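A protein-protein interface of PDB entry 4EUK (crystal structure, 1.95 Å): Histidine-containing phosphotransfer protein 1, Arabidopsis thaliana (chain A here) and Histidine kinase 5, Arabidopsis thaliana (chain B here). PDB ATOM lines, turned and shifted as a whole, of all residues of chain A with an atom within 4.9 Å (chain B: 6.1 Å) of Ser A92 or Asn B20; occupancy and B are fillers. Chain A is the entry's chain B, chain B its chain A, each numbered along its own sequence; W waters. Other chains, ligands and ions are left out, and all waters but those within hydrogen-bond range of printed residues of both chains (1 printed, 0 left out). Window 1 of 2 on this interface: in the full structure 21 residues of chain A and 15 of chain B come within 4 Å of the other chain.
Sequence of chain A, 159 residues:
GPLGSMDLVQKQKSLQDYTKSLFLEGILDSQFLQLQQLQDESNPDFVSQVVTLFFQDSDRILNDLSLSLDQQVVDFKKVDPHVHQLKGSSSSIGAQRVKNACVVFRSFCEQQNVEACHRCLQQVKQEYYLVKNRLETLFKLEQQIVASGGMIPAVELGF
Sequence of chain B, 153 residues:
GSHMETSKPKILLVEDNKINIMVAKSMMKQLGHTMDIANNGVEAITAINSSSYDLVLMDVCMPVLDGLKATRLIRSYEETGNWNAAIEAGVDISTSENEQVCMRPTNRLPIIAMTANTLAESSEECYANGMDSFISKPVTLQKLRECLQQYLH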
ATOM      1  N   GLN A  31     -16.279 -31.333  12.496  1.00  0.00           N
ATOM      2  CA  GLN A  31     -15.087 -31.512  11.647  1.00  0.00           C
ATOM      3  C   GLN A  31     -13.949 -32.207  12.390  1.00  0.00           C
ATOM      4  O   GLN A  31     -13.139 -32.932  11.784  1.00  0.00           O
ATOM      5  CB  GLN A  31     -14.627 -30.148  11.085  1.00  0.00           C
ATOM      6  CG  GLN A  31     -13.422 -30.210  10.156  1.00  0.00           C
ATOM      7  CD  GLN A  31     -13.720 -30.933   8.839  1.00  0.00           C
ATOM      8  OE1 GLN A  31     -14.879 -31.213   8.483  1.00  0.00           O
ATOM      9  NE2 GLN A  31     -12.668 -31.199   8.086  1.00  0.00           N
ATOM     10  N   LEU A  35     -11.486 -35.847  11.434  1.00  0.00           N
ATOM     11  CA  LEU A  35     -10.077 -36.163  11.631  1.00  0.00           C
ATOM     12  C   LEU A  35      -9.927 -37.479  12.394  1.00  0.00           C
ATOM     13  O   LEU A  35      -9.084 -38.317  12.044  1.00  0.00           O
ATOM     14  CB  LEU A  35      -9.341 -35.053  12.393  1.00  0.00           C
ATOM     15  CG  LEU A  35      -9.443 -33.619  11.884  1.00  0.00           C
ATOM     16  CD1 LEU A  35      -8.560 -32.693  12.724  1.00  0.00           C
ATOM     17  CD2 LEU A  35      -9.042 -33.546  10.425  1.00  0.00           C
ATOM     18  N   GLY A  88      -9.331 -20.445   8.159  1.00  0.00           N
ATOM     19  CA  GLY A  88      -9.341 -21.671   7.346  1.00  0.00           C
ATOM     20  C   GLY A  88      -8.800 -22.887   8.105  1.00  0.00           C
ATOM     21  O   GLY A  88      -9.395 -23.989   8.037  1.00  0.00           O
ATOM     22  N   SER A  89      -7.673 -22.700   8.775  1.00  0.00           N
ATOM     23  CA  SER A  89      -7.031 -23.786   9.524  1.00  0.00           C
ATOM     24  C   SER A  89      -7.921 -24.266  10.669  1.00  0.00           C
ATOM     25  O   SER A  89      -8.117 -25.493  10.857  1.00  0.00           O
ATOM     26  CB  SER A  89      -5.674 -23.338  10.058  1.00  0.00           C
ATOM     27  OG  SER A  89      -4.795 -23.016   9.002  1.00  0.00           O
ATOM     28  N   SER A  90      -8.484 -23.316  11.412  1.00  0.00           N
ATOM     29  CA  SER A  90      -9.416 -23.644  12.508  1.00  0.00           C
ATOM     30  C   SER A  90     -10.645 -24.371  12.019  1.00  0.00           C
ATOM     31  O   SER A  90     -11.095 -25.338  12.629  1.00  0.00           O
ATOM     32  CB  SER A  90      -9.866 -22.381  13.225  1.00  0.00           C
ATOM     33  OG  SER A  90      -8.750 -21.716  13.748  1.00  0.00           O
ATOM     34  N   SER A  91     -11.200 -23.902  10.893  1.00  0.00           N
ATOM     35  CA  SER A  91     -12.345 -24.532  10.302  1.00  0.00           C
ATOM     36  C   SER A  91     -12.043 -26.005   9.958  1.00  0.00           C
ATOM     37  O   SER A  91     -12.857 -26.906  10.203  1.00  0.00           O
ATOM     38  CB  SER A  91     -12.759 -23.736   9.033  1.00  0.00           C
ATOM     39  OG  SER A  91     -13.861 -24.330   8.390  1.00  0.00           O
ATOM     40  N   SER A  92     -10.871 -26.233   9.382  1.00  0.00           N
ATOM     41  CA  SER A  92     -10.493 -27.549   8.888  1.00  0.00           C
ATOM     42  C   SER A  92     -10.148 -28.539   9.996  1.00  0.00           C
ATOM     43  O   SER A  92     -10.169 -29.732   9.749  1.00  0.00           O
ATOM     44  CB  SER A  92      -9.345 -27.439   7.869  1.00  0.00           C
ATOM     45  OG  SER A  92      -9.830 -26.807   6.668  1.00  0.00           O
ATOM     46  N   ILE A  93      -9.857 -28.075  11.206  1.00  0.00           N
ATOM     47  CA  ILE A  93      -9.661 -29.047  12.316  1.00  0.00           C
ATOM     48  C   ILE A  93     -10.844 -29.066  13.288  1.00  0.00           C
ATOM     49  O   ILE A  93     -10.857 -29.869  14.216  1.00  0.00           O
ATOM     50  CB  ILE A  93      -8.358 -28.850  13.115  1.00  0.00           C
ATOM     51  CG1 ILE A  93      -8.381 -27.555  13.898  1.00  0.00           C
ATOM     52  CG2 ILE A  93      -7.090 -28.917  12.198  1.00  0.00           C
ATOM     53  CD1 ILE A  93      -7.496 -27.585  15.094  1.00  0.00           C
ATOM     54  N   GLY A  94     -11.803 -28.170  13.076  1.00  0.00           N
ATOM     55  CA  GLY A  94     -13.022 -28.108  13.877  1.00  0.00           C
ATOM     56  C   GLY A  94     -12.917 -27.306  15.167  1.00  0.00           C
ATOM     57  O   GLY A  94     -13.665 -27.584  16.119  1.00  0.00           O
ATOM     58  N   LEU B  13      -4.609 -31.356  -6.704  1.00  0.00           N
ATOM     59  CA  LEU B  13      -5.119 -30.505  -5.630  1.00  0.00           C
ATOM     60  C   LEU B  13      -4.361 -29.187  -5.637  1.00  0.00           C
ATOM     61  O   LEU B  13      -3.130 -29.179  -5.574  1.00  0.00           O
ATOM     62  CB  LEU B  13      -4.911 -31.190  -4.269  1.00  0.00           C
ATOM     63  CG  LEU B  13      -5.335 -30.363  -3.049  1.00  0.00           C
ATOM     64  CD1 LEU B  13      -6.846 -30.260  -3.022  1.00  0.00           C
ATOM     65  CD2 LEU B  13      -4.773 -30.941  -1.724  1.00  0.00           C
ATOM     66  N   GLU B  15      -4.122 -25.784  -3.528  1.00  0.00           N
ATOM     67  CA  GLU B  15      -4.480 -25.255  -2.218  1.00  0.00           C
ATOM     68  C   GLU B  15      -3.229 -24.654  -1.582  1.00  0.00           C
ATOM     69  O   GLU B  15      -2.134 -25.203  -1.692  1.00  0.00           O
ATOM     70  CB  GLU B  15      -5.122 -26.385  -1.391  1.00  0.00           C
ATOM     71  CG  GLU B  15      -5.264 -26.185   0.067  1.00  0.00           C
ATOM     72  CD  GLU B  15      -6.278 -25.138   0.462  1.00  0.00           C
ATOM     73  OE1 GLU B  15      -7.497 -25.402   0.349  1.00  0.00           O
ATOM     74  OE2 GLU B  15      -5.845 -24.062   0.941  1.00  0.00           O
ATOM     75  N   ASN B  17      -3.176 -23.615   1.769  1.00  0.00           N
ATOM     76  CA  ASN B  17      -3.117 -23.821   3.219  1.00  0.00           C
ATOM     77  C   ASN B  17      -2.629 -25.239   3.527  1.00  0.00           C
ATOM     78  O   ASN B  17      -3.273 -26.211   3.162  1.00  0.00           O
ATOM     79  CB  ASN B  17      -4.489 -23.511   3.841  1.00  0.00           C
ATOM     80  CG  ASN B  17      -4.540 -23.712   5.350  1.00  0.00           C
ATOM     81  OD1 ASN B  17      -4.116 -24.748   5.866  1.00  0.00           O
ATOM     82  ND2 ASN B  17      -5.131 -22.732   6.066  1.00  0.00           N
ATOM     83  N   LYS B  18      -1.510 -25.349   4.238  1.00  0.00           N
ATOM     84  CA  LYS B  18      -0.889 -26.661   4.515  1.00  0.00           C
ATOM     85  C   LYS B  18      -1.720 -27.599   5.390  1.00  0.00           C
ATOM     86  O   LYS B  18      -1.649 -28.814   5.237  1.00  0.00           O
ATOM     87  CB  LYS B  18       0.485 -26.487   5.172  1.00  0.00           C
ATOM     88  CG  LYS B  18       1.483 -25.646   4.371  1.00  0.00           C
ATOM     89  CD  LYS B  18       1.728 -26.189   2.975  1.00  0.00           C
ATOM     90  CE  LYS B  18       2.946 -25.496   2.338  1.00  0.00           C
ATOM     91  NZ  LYS B  18       2.991 -25.727   0.880  1.00  0.00           N
ATOM     92  N   ILE B  19      -2.478 -27.043   6.334  1.00  0.00           N
ATOM     93  CA  ILE B  19      -3.397 -27.836   7.133  1.00  0.00           C
ATOM     94  C   ILE B  19      -4.482 -28.409   6.231  1.00  0.00           C
ATOM     95  O   ILE B  19      -4.770 -29.616   6.284  1.00  0.00           O
ATOM     96  CB  ILE B  19      -4.013 -27.033   8.331  1.00  0.00           C
ATOM     97  CG1 ILE B  19      -2.975 -26.817   9.428  1.00  0.00           C
ATOM     98  CG2 ILE B  19      -5.189 -27.768   8.940  1.00  0.00           C
ATOM     99  CD1 ILE B  19      -2.001 -25.741   9.126  1.00  0.00           C
ATOM    100  N   ASN B  20      -5.062 -27.561   5.370  1.00  0.00           N
ATOM    101  CA  ASN B  20      -6.075 -28.035   4.436  1.00  0.00           C
ATOM    102  C   ASN B  20      -5.520 -29.156   3.540  1.00  0.00           C
ATOM    103  O   ASN B  20      -6.204 -30.119   3.257  1.00  0.00           O
ATOM    104  CB  ASN B  20      -6.581 -26.897   3.543  1.00  0.00           C
ATOM    105  CG  ASN B  20      -7.402 -25.833   4.290  1.00  0.00           C
ATOM    106  OD1 ASN B  20      -7.825 -24.826   3.681  1.00  0.00           O
ATOM    107  ND2 ASN B  20      -7.628 -26.029   5.575  1.00  0.00           N
ATOM    108  N   ILE B  21      -4.274 -29.027   3.100  1.00  0.00           N
ATOM    109  CA  ILE B  21      -3.662 -30.060   2.248  1.00  0.00           C
ATOM    110  C   ILE B  21      -3.554 -31.401   2.988  1.00  0.00           C
ATOM    111  O   ILE B  21      -3.908 -32.446   2.446  1.00  0.00           O
ATOM    112  CB  ILE B  21      -2.290 -29.636   1.687  1.00  0.00           C
ATOM    113  CG1 ILE B  21      -2.423 -28.513   0.641  1.00  0.00           C
ATOM    114  CG2 ILE B  21      -1.541 -30.843   1.040  1.00  0.00           C
ATOM    115  CD1 ILE B  21      -1.107 -27.753   0.341  1.00  0.00           C
ATOM    116  N   MET B  22      -3.064 -31.377   4.227  1.00  0.00           N
ATOM    117  CA  MET B  22      -2.857 -32.624   4.979  1.00  0.00           C
ATOM    118  C   MET B  22      -4.186 -33.344   5.173  1.00  0.00           C
ATOM    119  O   MET B  22      -4.281 -34.562   4.973  1.00  0.00           O
ATOM    120  CB  MET B  22      -2.171 -32.375   6.329  1.00  0.00           C
ATOM    121  CG  MET B  22      -1.950 -33.664   7.123  1.00  0.00           C
ATOM    122  SD  MET B  22      -1.012 -33.479   8.637  1.00  0.00           S
ATOM    123  CE  MET B  22      -0.444 -35.166   8.881  1.00  0.00           C
ATOM    124  N   VAL B  23      -5.229 -32.593   5.512  1.00  0.00           N
ATOM    125  CA  VAL B  23      -6.546 -33.189   5.716  1.00  0.00           C
ATOM    126  C   VAL B  23      -7.114 -33.778   4.399  1.00  0.00           C
ATOM    127  O   VAL B  23      -7.533 -34.941   4.380  1.00  0.00           O
ATOM    128  CB  VAL B  23      -7.508 -32.187   6.331  1.00  0.00           C
ATOM    129  CG1 VAL B  23      -8.889 -32.785   6.458  1.00  0.00           C
ATOM    130  CG2 VAL B  23      -6.978 -31.735   7.740  1.00  0.00           C
ATOM    131  N   ALA B  24      -7.076 -33.004   3.307  1.00  0.00           N
ATOM    132  CA  ALA B  24      -7.598 -33.466   2.000  1.00  0.00           C
ATOM    133  C   ALA B  24      -6.827 -34.673   1.468  1.00  0.00           C
ATOM    134  O   ALA B  24      -7.417 -35.627   0.944  1.00  0.00           O
ATOM    135  CB  ALA B  24      -7.613 -32.312   0.963  1.00  0.00           C
ATOM    136  N   LYS B  25      -5.511 -34.661   1.634  1.00  0.00           N
ATOM    137  CA  LYS B  25      -4.673 -35.813   1.259  1.00  0.00           C
ATOM    138  C   LYS B  25      -5.071 -37.121   1.924  1.00  0.00           C
ATOM    139  O   LYS B  25      -5.136 -38.161   1.264  1.00  0.00           O
ATOM    140  CB  LYS B  25      -3.201 -35.575   1.608  1.00  0.00           C
ATOM    141  CG  LYS B  25      -2.312 -35.025   0.521  1.00  0.00           C
ATOM    142  CD  LYS B  25      -0.867 -34.927   1.079  1.00  0.00           C
ATOM    143  CE  LYS B  25       0.189 -34.801  -0.002  1.00  0.00           C
ATOM    144  NZ  LYS B  25       1.570 -34.742   0.601  1.00  0.00           N
ATOM    145  N   ASP B  59      -8.689 -24.535  -5.047  1.00  0.00           N
ATOM    146  CA  ASP B  59      -8.992 -23.554  -4.018  1.00  0.00           C
ATOM    147  C   ASP B  59      -9.272 -22.230  -4.718  1.00  0.00           C
ATOM    148  O   ASP B  59      -8.659 -21.911  -5.743  1.00  0.00           O
ATOM    149  CB  ASP B  59      -7.793 -23.417  -3.097  1.00  0.00           C
ATOM    150  CG  ASP B  59      -8.056 -22.557  -1.866  1.00  0.00           C
ATOM    151  OD1 ASP B  59      -9.212 -22.413  -1.410  1.00  0.00           O
ATOM    152  OD2 ASP B  59      -7.056 -22.059  -1.329  1.00  0.00           O
ATOM    153  N   LYS B 137     -16.019 -25.508   2.010  1.00  0.00           N
ATOM    154  CA  LYS B 137     -15.082 -25.916   3.055  1.00  0.00           C
ATOM    155  C   LYS B 137     -15.778 -25.845   4.405  1.00  0.00           C
ATOM    156  O   LYS B 137     -16.660 -25.030   4.590  1.00  0.00           O
ATOM    157  CB  LYS B 137     -13.853 -25.021   3.072  1.00  0.00           C
ATOM    158  CG  LYS B 137     -12.953 -25.233   1.900  1.00  0.00           C
ATOM    159  CD  LYS B 137     -11.903 -24.094   1.891  1.00  0.00           C
ATOM    160  CE  LYS B 137     -10.776 -24.308   0.962  1.00  0.00           C
ATOM    161  NZ  LYS B 137      -9.721 -23.232   1.091  1.00  0.00           N
ATOM    162  N   PRO B 138     -15.353 -26.654   5.377  1.00  0.00           N
ATOM    163  CA  PRO B 138     -14.246 -27.579   5.351  1.00  0.00           C
ATOM    164  C   PRO B 138     -14.572 -28.826   4.530  1.00  0.00           C
ATOM    165  O   PRO B 138     -15.714 -29.300   4.543  1.00  0.00           O
ATOM    166  CB  PRO B 138     -14.054 -27.926   6.855  1.00  0.00           C
ATOM    167  CG  PRO B 138     -15.430 -27.806   7.424  1.00  0.00           C
ATOM    168  CD  PRO B 138     -16.042 -26.644   6.688  1.00  0.00           C
ATOM    169  N   VAL B 139     -13.585 -29.354   3.805  1.00  0.00           N
ATOM    170  CA  VAL B 139     -13.781 -30.591   3.042  1.00  0.00           C
ATOM    171  C   VAL B 139     -14.052 -31.762   3.989  1.00  0.00           C
ATOM    172  O   VAL B 139     -13.450 -31.855   5.044  1.00  0.00           O
ATOM    173  CB  VAL B 139     -12.561 -30.860   2.105  1.00  0.00           C
ATOM    174  CG1 VAL B 139     -12.764 -32.104   1.281  1.00  0.00           C
ATOM    175  CG2 VAL B 139     -12.360 -29.656   1.173  1.00  0.00           C
HETATM  176  O   HOH W   1     -10.993 -28.083   4.265  1.00  0.00           O
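Among the printed residues, pairs that only touch across the chains: Ser A91 with Pro B138, Gln A31 with Pro B138, Gly A88 with Asn B20, Leu A35 with Val B23, Ser A89 with Ile B19 and Ile A93 with Ile B19.
Printed residues of chain A that touch a printed residue of chain B: Gln A31, Leu A35, Gly A88, Ser A89, Ser A91, Ser A92 and Ile A93. Hydrophobic or aromatic side chains of chain B that line the printed part of chain A: Ile B19, Val B23 and Pro B138. Along chain B the printed residues that touch a printed residue of chain A span positions 17 to 139. Among the printed residues, no Asp or Glu carboxylate lies within 4 Å of a Lys or Arg side-chain nitrogen of the other chain.
ND2 of Asn B17 is in hydrogen-bond range of OG of Ser A89 (3.0 Å). The side-chain amide nitrogen (ND2) of Asn B20 sits at hydrogen-bond distance from the side-chain hydroxyl (OG) of Ser A92 (2.6 Å). The backbone carbonyl oxygen of Val B139 is in hydrogen-bond range of the side-chain amide nitrogen of Gln A31, 3.2 Å away.
Of the printed residues of chain B, Gln A31 touches Pro B138 (3.6 Å) and Val B139 (3.2 Å). Of the printed residues of chain B, Leu A35 touches Val B23. Of chain B, only Asn B20 comes within 4 Å of Ser A92. Of the printed residues of chain A, Asn B17 touches Ser A89. Of chain A, only Gly A88 and Ser A92 come within 4 Å of Asn B20. Printed residues of chain A within 4 Å of Val B23: Leu A35. The nearest residue of chain B that does not touch Ser A92 is Pro B138 (4.1 Å).
Water W1 bridges the backbone NH of Val B139 (2.9 Å) and the side-chain hydroxyl of Ser A92 (3.0 Å).
The side-chain amide oxygen (OD1) of Asn B20 lies close to the side-chain carboxylate (OE1) of Glu B15, 3.4 Å away. N of Asn B17 lies within hydrogen-bond range of OE2 of Glu B15, at 2.8 Å. The side-chain hydroxyl of Ser A92 lies within hydrogen-bond range of the backbone carbonyl oxygen of Gly A88, 3.2 Å away. The backbone NH of Ile B19 is in hydrogen-bond range of the side-chain amide oxygen of Asn B17 (2.9 Å). OD1 of Asn B17 is in hydrogen-bond range of N of Asn B20, at 3.0 Å. NE2 of Gln A31 lies close to O of Ser A92 (3.3 Å).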
